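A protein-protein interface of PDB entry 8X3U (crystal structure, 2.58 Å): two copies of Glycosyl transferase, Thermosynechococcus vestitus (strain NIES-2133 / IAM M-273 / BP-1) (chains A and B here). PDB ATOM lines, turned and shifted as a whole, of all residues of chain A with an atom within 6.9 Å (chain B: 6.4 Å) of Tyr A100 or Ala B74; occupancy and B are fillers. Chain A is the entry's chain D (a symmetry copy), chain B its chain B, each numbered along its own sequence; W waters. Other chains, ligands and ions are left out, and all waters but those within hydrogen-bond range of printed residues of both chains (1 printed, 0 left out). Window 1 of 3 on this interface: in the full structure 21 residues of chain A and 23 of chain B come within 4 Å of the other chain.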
ATOM      1  N   GLU A  77     -29.659  26.237 -16.163  1.00  0.00           N
ATOM      2  CA  GLU A  77     -29.296  25.582 -17.414  1.00  0.00           C
ATOM      3  C   GLU A  77     -27.961  24.857 -17.282  1.00  0.00           C
ATOM      4  O   GLU A  77     -27.820  23.705 -17.706  1.00  0.00           O
ATOM      5  CB  GLU A  77     -29.248  26.614 -18.540  1.00  0.00           C
ATOM      6  CG  GLU A  77     -29.226  26.027 -19.934  1.00  0.00           C
ATOM      7  CD  GLU A  77     -28.963  27.082 -20.981  1.00  0.00           C
ATOM      8  OE1 GLU A  77     -28.491  28.174 -20.603  1.00  0.00           O
ATOM      9  OE2 GLU A  77     -29.224  26.822 -22.175  1.00  0.00           O
ATOM     10  N   LEU A  81     -27.195  20.820 -17.481  1.00  0.00           N
ATOM     11  CA  LEU A  81     -26.228  20.238 -18.406  1.00  0.00           C
ATOM     12  C   LEU A  81     -25.125  19.492 -17.666  1.00  0.00           C
ATOM     13  O   LEU A  81     -24.631  18.470 -18.155  1.00  0.00           O
ATOM     14  CB  LEU A  81     -25.645  21.328 -19.304  1.00  0.00           C
ATOM     15  CG  LEU A  81     -26.648  21.880 -20.321  1.00  0.00           C
ATOM     16  CD1 LEU A  81     -26.023  22.956 -21.201  1.00  0.00           C
ATOM     17  CD2 LEU A  81     -27.223  20.750 -21.167  1.00  0.00           C
ATOM     18  N   SER A  96     -30.984  16.377 -26.858  1.00  0.00           N
ATOM     19  CA  SER A  96     -30.919  17.735 -26.339  1.00  0.00           C
ATOM     20  C   SER A  96     -31.842  18.661 -27.118  1.00  0.00           C
ATOM     21  O   SER A  96     -31.883  18.629 -28.352  1.00  0.00           O
ATOM     22  CB  SER A  96     -29.488  18.273 -26.396  1.00  0.00           C
ATOM     23  OG  SER A  96     -29.448  19.629 -25.987  1.00  0.00           O
ATOM     24  N   VAL A  98     -31.941  22.081 -25.889  1.00  0.00           N
ATOM     25  CA  VAL A  98     -31.568  23.347 -25.265  1.00  0.00           C
ATOM     26  C   VAL A  98     -30.665  24.185 -26.162  1.00  0.00           C
ATOM     27  O   VAL A  98     -30.162  25.227 -25.730  1.00  0.00           O
ATOM     28  CB  VAL A  98     -30.908  23.115 -23.896  1.00  0.00           C
ATOM     29  CG1 VAL A  98     -31.766  22.197 -23.041  1.00  0.00           C
ATOM     30  CG2 VAL A  98     -29.509  22.539 -24.069  1.00  0.00           C
ATOM     31  N   GLY A  99     -30.457  23.763 -27.406  1.00  0.00           N
ATOM     32  CA  GLY A  99     -29.703  24.573 -28.345  1.00  0.00           C
ATOM     33  C   GLY A  99     -28.200  24.374 -28.242  1.00  0.00           C
ATOM     34  O   GLY A  99     -27.707  23.326 -27.822  1.00  0.00           O
ATOM     35  N   TYR A 100     -27.467  25.427 -28.617  1.00  0.00           N
ATOM     36  CA  TYR A 100     -26.028  25.321 -28.836  1.00  0.00           C
ATOM     37  C   TYR A 100     -25.239  25.129 -27.550  1.00  0.00           C
ATOM     38  O   TYR A 100     -24.084  24.696 -27.612  1.00  0.00           O
ATOM     39  CB  TYR A 100     -25.519  26.572 -29.558  1.00  0.00           C
ATOM     40  CG  TYR A 100     -25.749  27.861 -28.795  1.00  0.00           C
ATOM     41  CD1 TYR A 100     -24.862  28.275 -27.807  1.00  0.00           C
ATOM     42  CD2 TYR A 100     -26.848  28.666 -29.066  1.00  0.00           C
ATOM     43  CE1 TYR A 100     -25.068  29.449 -27.107  1.00  0.00           C
ATOM     44  CE2 TYR A 100     -27.061  29.845 -28.372  1.00  0.00           C
ATOM     45  CZ  TYR A 100     -26.167  30.230 -27.393  1.00  0.00           C
ATOM     46  OH  TYR A 100     -26.366  31.399 -26.694  1.00  0.00           O
ATOM     47  N   THR A 101     -25.825  25.451 -26.393  1.00  0.00           N
ATOM     48  CA  THR A 101     -25.109  25.380 -25.123  1.00  0.00           C
ATOM     49  C   THR A 101     -24.632  23.974 -24.781  1.00  0.00           C
ATOM     50  O   THR A 101     -23.835  23.822 -23.849  1.00  0.00           O
ATOM     51  CB  THR A 101     -25.995  25.912 -23.994  1.00  0.00           C
ATOM     52  OG1 THR A 101     -27.076  25.002 -23.764  1.00  0.00           O
ATOM     53  CG2 THR A 101     -26.568  27.273 -24.361  1.00  0.00           C
ATOM     54  N   ALA A 102     -25.093  22.952 -25.502  1.00  0.00           N
ATOM     55  CA  ALA A 102     -24.713  21.572 -25.236  1.00  0.00           C
ATOM     56  C   ALA A 102     -23.650  21.041 -26.189  1.00  0.00           C
ATOM     57  O   ALA A 102     -23.145  19.935 -25.971  1.00  0.00           O
ATOM     58  CB  ALA A 102     -25.948  20.665 -25.305  1.00  0.00           C
ATOM     59  N   LEU A 103     -23.293  21.802 -27.225  1.00  0.00           N
ATOM     60  CA  LEU A 103     -22.332  21.313 -28.210  1.00  0.00           C
ATOM     61  C   LEU A 103     -20.949  21.064 -27.621  1.00  0.00           C
ATOM     62  O   LEU A 103     -20.375  19.994 -27.897  1.00  0.00           O
ATOM     63  CB  LEU A 103     -22.272  22.277 -29.398  1.00  0.00           C
ATOM     64  CG  LEU A 103     -23.613  22.613 -30.048  1.00  0.00           C
ATOM     65  CD1 LEU A 103     -23.386  23.393 -31.327  1.00  0.00           C
ATOM     66  CD2 LEU A 103     -24.412  21.352 -30.318  1.00  0.00           C
ATOM     67  N   PRO A 104     -20.346  21.971 -26.843  1.00  0.00           N
ATOM     68  CA  PRO A 104     -19.026  21.658 -26.274  1.00  0.00           C
ATOM     69  C   PRO A 104     -19.044  20.463 -25.341  1.00  0.00           C
ATOM     70  O   PRO A 104     -17.998  19.834 -25.143  1.00  0.00           O
ATOM     71  CB  PRO A 104     -18.637  22.946 -25.531  1.00  0.00           C
ATOM     72  CG  PRO A 104     -19.883  23.746 -25.428  1.00  0.00           C
ATOM     73  CD  PRO A 104     -20.739  23.367 -26.575  1.00  0.00           C
ATOM     74  N   TYR A 105     -20.201  20.120 -24.767  1.00  0.00           N
ATOM     75  CA  TYR A 105     -20.274  18.937 -23.920  1.00  0.00           C
ATOM     76  C   TYR A 105     -20.207  17.657 -24.741  1.00  0.00           C
ATOM     77  O   TYR A 105     -19.701  16.637 -24.257  1.00  0.00           O
ATOM     78  CB  TYR A 105     -21.563  18.949 -23.101  1.00  0.00           C
ATOM     79  CG  TYR A 105     -21.609  19.998 -22.018  1.00  0.00           C
ATOM     80  CD1 TYR A 105     -20.922  19.824 -20.826  1.00  0.00           C
ATOM     81  CD2 TYR A 105     -22.345  21.164 -22.188  1.00  0.00           C
ATOM     82  CE1 TYR A 105     -20.964  20.783 -19.832  1.00  0.00           C
ATOM     83  CE2 TYR A 105     -22.393  22.128 -21.201  1.00  0.00           C
ATOM     84  CZ  TYR A 105     -21.701  21.932 -20.025  1.00  0.00           C
ATOM     85  OH  TYR A 105     -21.743  22.889 -19.037  1.00  0.00           O
ATOM     86  N   HIS A 115     -29.072  16.540 -31.340  1.00  0.00           N
ATOM     87  CA  HIS A 115     -29.539  17.903 -31.096  1.00  0.00           C
ATOM     88  C   HIS A 115     -30.703  18.220 -32.029  1.00  0.00           C
ATOM     89  O   HIS A 115     -30.529  18.259 -33.251  1.00  0.00           O
ATOM     90  CB  HIS A 115     -28.403  18.904 -31.296  1.00  0.00           C
ATOM     91  CG  HIS A 115     -27.190  18.614 -30.466  1.00  0.00           C
ATOM     92  ND1 HIS A 115     -26.124  17.879 -30.936  1.00  0.00           N
ATOM     93  CD2 HIS A 115     -26.875  18.963 -29.196  1.00  0.00           C
ATOM     94  CE1 HIS A 115     -25.205  17.786 -29.993  1.00  0.00           C
ATOM     95  NE2 HIS A 115     -25.637  18.435 -28.927  1.00  0.00           N
ATOM     96  N   LEU A 117     -32.759  21.083 -33.390  1.00  0.00           N
ATOM     97  CA  LEU A 117     -32.746  22.532 -33.541  1.00  0.00           C
ATOM     98  C   LEU A 117     -34.173  23.066 -33.490  1.00  0.00           C
ATOM     99  O   LEU A 117     -35.002  22.722 -34.342  1.00  0.00           O
ATOM    100  CB  LEU A 117     -32.068  22.917 -34.854  1.00  0.00           C
ATOM    101  CG  LEU A 117     -30.703  22.260 -35.067  1.00  0.00           C
ATOM    102  CD1 LEU A 117     -30.345  22.200 -36.545  1.00  0.00           C
ATOM    103  CD2 LEU A 117     -29.627  22.995 -34.272  1.00  0.00           C
ATOM    104  N   ASN A 125     -24.940  32.619 -33.899  1.00  0.00           N
ATOM    105  CA  ASN A 125     -24.996  31.194 -33.573  1.00  0.00           C
ATOM    106  C   ASN A 125     -24.476  30.310 -34.703  1.00  0.00           C
ATOM    107  O   ASN A 125     -24.106  29.159 -34.451  1.00  0.00           O
ATOM    108  CB  ASN A 125     -26.419  30.779 -33.161  1.00  0.00           C
ATOM    109  CG  ASN A 125     -27.399  30.656 -34.335  1.00  0.00           C
ATOM    110  OD1 ASN A 125     -27.039  30.762 -35.509  1.00  0.00           O
ATOM    111  ND2 ASN A 125     -28.661  30.418 -33.999  1.00  0.00           N
ATOM    112  N   ILE A 128     -20.901  28.890 -33.818  1.00  0.00           N
ATOM    113  CA  ILE A 128     -20.717  27.744 -32.928  1.00  0.00           C
ATOM    114  C   ILE A 128     -21.173  26.447 -33.589  1.00  0.00           C
ATOM    115  O   ILE A 128     -20.573  25.387 -33.373  1.00  0.00           O
ATOM    116  CB  ILE A 128     -21.431  27.979 -31.582  1.00  0.00           C
ATOM    117  CG1 ILE A 128     -21.176  26.807 -30.633  1.00  0.00           C
ATOM    118  CG2 ILE A 128     -22.926  28.160 -31.774  1.00  0.00           C
ATOM    119  CD1 ILE A 128     -21.531  27.097 -29.191  1.00  0.00           C
ATOM    120  N   PHE A 129     -22.227  26.498 -34.408  1.00  0.00           N
ATOM    121  CA  PHE A 129     -22.664  25.293 -35.112  1.00  0.00           C
ATOM    122  C   PHE A 129     -21.651  24.863 -36.166  1.00  0.00           C
ATOM    123  O   PHE A 129     -21.386  23.664 -36.322  1.00  0.00           O
ATOM    124  CB  PHE A 129     -24.038  25.521 -35.740  1.00  0.00           C
ATOM    125  CG  PHE A 129     -25.163  25.521 -34.743  1.00  0.00           C
ATOM    126  CD1 PHE A 129     -25.437  24.392 -33.993  1.00  0.00           C
ATOM    127  CD2 PHE A 129     -25.943  26.650 -34.556  1.00  0.00           C
ATOM    128  CE1 PHE A 129     -26.466  24.387 -33.071  1.00  0.00           C
ATOM    129  CE2 PHE A 129     -26.976  26.652 -33.640  1.00  0.00           C
ATOM    130  CZ  PHE A 129     -27.237  25.520 -32.896  1.00  0.00           C
ATOM    131  N   TYR A 132     -18.985  22.761 -34.800  1.00  0.00           N
ATOM    132  CA  TYR A 132     -19.423  21.433 -34.381  1.00  0.00           C
ATOM    133  C   TYR A 132     -20.330  20.791 -35.426  1.00  0.00           C
ATOM    134  O   TYR A 132     -21.273  20.067 -35.095  1.00  0.00           O
ATOM    135  CB  TYR A 132     -20.128  21.501 -33.029  1.00  0.00           C
ATOM    136  CG  TYR A 132     -19.230  21.925 -31.885  1.00  0.00           C
ATOM    137  CD1 TYR A 132     -18.284  21.055 -31.359  1.00  0.00           C
ATOM    138  CD2 TYR A 132     -19.327  23.198 -31.333  1.00  0.00           C
ATOM    139  CE1 TYR A 132     -17.462  21.438 -30.315  1.00  0.00           C
ATOM    140  CE2 TYR A 132     -18.508  23.590 -30.290  1.00  0.00           C
ATOM    141  CZ  TYR A 132     -17.578  22.704 -29.784  1.00  0.00           C
ATOM    142  OH  TYR A 132     -16.760  23.085 -28.746  1.00  0.00           O
ATOM    143  N   TRP B  13     -15.905  39.982 -22.871  1.00  0.00           N
ATOM    144  CA  TRP B  13     -16.504  41.307 -22.974  1.00  0.00           C
ATOM    145  C   TRP B  13     -15.460  42.359 -23.321  1.00  0.00           C
ATOM    146  O   TRP B  13     -15.754  43.317 -24.045  1.00  0.00           O
ATOM    147  CB  TRP B  13     -17.223  41.659 -21.674  1.00  0.00           C
ATOM    148  CG  TRP B  13     -18.430  40.806 -21.419  1.00  0.00           C
ATOM    149  CD1 TRP B  13     -18.540  39.788 -20.515  1.00  0.00           C
ATOM    150  CD2 TRP B  13     -19.699  40.892 -22.080  1.00  0.00           C
ATOM    151  NE1 TRP B  13     -19.798  39.238 -20.571  1.00  0.00           N
ATOM    152  CE2 TRP B  13     -20.529  39.899 -21.525  1.00  0.00           C
ATOM    153  CE3 TRP B  13     -20.214  41.715 -23.087  1.00  0.00           C
ATOM    154  CZ2 TRP B  13     -21.844  39.706 -21.941  1.00  0.00           C
ATOM    155  CZ3 TRP B  13     -21.521  41.522 -23.500  1.00  0.00           C
ATOM    156  CH2 TRP B  13     -22.321  40.527 -22.927  1.00  0.00           C
ATOM    157  N   GLU B  72     -25.047  37.830 -29.340  1.00  0.00           N
ATOM    158  CA  GLU B  72     -25.176  36.686 -28.435  1.00  0.00           C
ATOM    159  C   GLU B  72     -23.795  36.341 -27.881  1.00  0.00           C
ATOM    160  O   GLU B  72     -23.090  35.497 -28.443  1.00  0.00           O
ATOM    161  CB  GLU B  72     -25.816  35.504 -29.158  1.00  0.00           C
ATOM    162  CG  GLU B  72     -27.256  35.759 -29.588  1.00  0.00           C
ATOM    163  CD  GLU B  72     -27.747  34.757 -30.611  1.00  0.00           C
ATOM    164  OE1 GLU B  72     -27.142  33.671 -30.722  1.00  0.00           O
ATOM    165  OE2 GLU B  72     -28.737  35.057 -31.311  1.00  0.00           O
ATOM    166  N   TYR B  73     -23.412  37.008 -26.788  1.00  0.00           N
ATOM    167  CA  TYR B  73     -22.115  36.754 -26.165  1.00  0.00           C
ATOM    168  C   TYR B  73     -21.968  35.298 -25.736  1.00  0.00           C
ATOM    169  O   TYR B  73     -20.882  34.718 -25.856  1.00  0.00           O
ATOM    170  CB  TYR B  73     -21.932  37.697 -24.972  1.00  0.00           C
ATOM    171  CG  TYR B  73     -20.787  37.373 -24.026  1.00  0.00           C
ATOM    172  CD1 TYR B  73     -20.953  36.472 -22.978  1.00  0.00           C
ATOM    173  CD2 TYR B  73     -19.556  38.003 -24.154  1.00  0.00           C
ATOM    174  CE1 TYR B  73     -19.917  36.184 -22.105  1.00  0.00           C
ATOM    175  CE2 TYR B  73     -18.512  37.725 -23.283  1.00  0.00           C
ATOM    176  CZ  TYR B  73     -18.700  36.814 -22.261  1.00  0.00           C
ATOM    177  OH  TYR B  73     -17.674  36.533 -21.387  1.00  0.00           O
ATOM    178  N   ALA B  74     -23.048  34.690 -25.231  1.00  0.00           N
ATOM    179  CA  ALA B  74     -22.963  33.323 -24.718  1.00  0.00           C
ATOM    180  C   ALA B  74     -22.471  32.340 -25.774  1.00  0.00           C
ATOM    181  O   ALA B  74     -21.892  31.301 -25.429  1.00  0.00           O
ATOM    182  CB  ALA B  74     -24.318  32.876 -24.176  1.00  0.00           C
ATOM    183  N   VAL B  75     -22.677  32.650 -27.057  1.00  0.00           N
ATOM    184  CA  VAL B  75     -22.235  31.753 -28.123  1.00  0.00           C
ATOM    185  C   VAL B  75     -20.720  31.601 -28.090  1.00  0.00           C
ATOM    186  O   VAL B  75     -20.184  30.487 -28.139  1.00  0.00           O
ATOM    187  CB  VAL B  75     -22.719  32.268 -29.492  1.00  0.00           C
ATOM    188  CG1 VAL B  75     -22.054  31.495 -30.615  1.00  0.00           C
ATOM    189  CG2 VAL B  75     -24.232  32.169 -29.599  1.00  0.00           C
ATOM    190  N   TYR B  76     -20.009  32.724 -27.996  1.00  0.00           N
ATOM    191  CA  TYR B  76     -18.552  32.703 -28.046  1.00  0.00           C
ATOM    192  C   TYR B  76     -17.950  32.262 -26.721  1.00  0.00           C
ATOM    193  O   TYR B  76     -16.856  31.689 -26.700  1.00  0.00           O
ATOM    194  CB  TYR B  76     -18.040  34.080 -28.468  1.00  0.00           C
ATOM    195  CG  TYR B  76     -18.662  34.526 -29.771  1.00  0.00           C
ATOM    196  CD1 TYR B  76     -19.876  35.202 -29.789  1.00  0.00           C
ATOM    197  CD2 TYR B  76     -18.053  34.237 -30.983  1.00  0.00           C
ATOM    198  CE1 TYR B  76     -20.456  35.594 -30.980  1.00  0.00           C
ATOM    199  CE2 TYR B  76     -18.626  34.627 -32.179  1.00  0.00           C
ATOM    200  CZ  TYR B  76     -19.826  35.303 -32.172  1.00  0.00           C
ATOM    201  OH  TYR B  76     -20.397  35.690 -33.360  1.00  0.00           O
ATOM    202  N   GLU B  77     -18.640  32.536 -25.613  1.00  0.00           N
ATOM    203  CA  GLU B  77     -18.268  31.952 -24.331  1.00  0.00           C
ATOM    204  C   GLU B  77     -18.238  30.427 -24.412  1.00  0.00           C
ATOM    205  O   GLU B  77     -17.296  29.786 -23.935  1.00  0.00           O
ATOM    206  CB  GLU B  77     -19.244  32.424 -23.253  1.00  0.00           C
ATOM    207  CG  GLU B  77     -18.871  32.051 -21.833  1.00  0.00           C
ATOM    208  CD  GLU B  77     -19.868  32.596 -20.825  1.00  0.00           C
ATOM    209  OE1 GLU B  77     -21.086  32.505 -21.092  1.00  0.00           O
ATOM    210  OE2 GLU B  77     -19.436  33.118 -19.775  1.00  0.00           O
ATOM    211  N   ALA B  78     -19.270  29.830 -25.019  1.00  0.00           N
ATOM    212  CA  ALA B  78     -19.310  28.376 -25.164  1.00  0.00           C
ATOM    213  C   ALA B  78     -18.206  27.879 -26.089  1.00  0.00           C
ATOM    214  O   ALA B  78     -17.610  26.822 -25.845  1.00  0.00           O
ATOM    215  CB  ALA B  78     -20.682  27.936 -25.675  1.00  0.00           C
ATOM    216  N   LEU B  79     -17.942  28.612 -27.174  1.00  0.00           N
ATOM    217  CA  LEU B  79     -16.804  28.297 -28.032  1.00  0.00           C
ATOM    218  C   LEU B  79     -15.508  28.260 -27.231  1.00  0.00           C
ATOM    219  O   LEU B  79     -14.674  27.366 -27.420  1.00  0.00           O
ATOM    220  CB  LEU B  79     -16.715  29.305 -29.178  1.00  0.00           C
ATOM    221  CG  LEU B  79     -17.667  29.068 -30.354  1.00  0.00           C
ATOM    222  CD1 LEU B  79     -17.872  30.348 -31.146  1.00  0.00           C
ATOM    223  CD2 LEU B  79     -17.146  27.960 -31.251  1.00  0.00           C
HETATM  224  O   HOH W   1     -27.610  32.972 -28.066  1.00  0.00           O
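Of the 17 printed residues of chain A, 4 touch a printed residue of chain B. Printed residues of chain A that touch a printed residue of chain B: Tyr A100, Pro A104, Asn A125 and Ile A128. Among the printed residues, no Asp or Glu carboxylate lies within 4 Å of a Lys or Arg side-chain nitrogen of the other chain.
1 position is printed for both chains.
Among the printed residues, merely in contact across the chains: Tyr A100 with Val B75, Tyr A100 with Ala B74, Ile A128 with Val B75, Ile A128 with Ala B78, Pro A104 with Ala B78, Asn A125 with Glu B72 and Ile A128 with Leu B79.
Water W1 lies within hydrogen-bond range of the side-chain hydroxyl of Tyr A100 (2.4 Å) and the side-chain carboxylate of Glu B72 (2.8 Å).
Tyr A100 touches two residues of chain B. Of chain A, only Tyr A100 comes within 4 Å of Ala B74. Printed residues of chain A within 4 Å of Leu B79: Ile A128. Of the printed residues of chain A, Glu B72 touches Asn A125 (3.9 Å). Of the printed residues of chain B, Pro A104 touches Ala B78 (3.8 Å). Of the printed residues of chain A, Val B75 touches Tyr A100 and Ile A128. Tyr B73 touches none of the printed residues of chain A. Tyr A132 touches none of the printed residues of chain B. The nearest residue of chain B that does not touch Tyr A100 is Glu B72 (4.5 Å). The nearest residue of chain A that does not touch Ala B74 is Ile A128 (5.7 Å).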
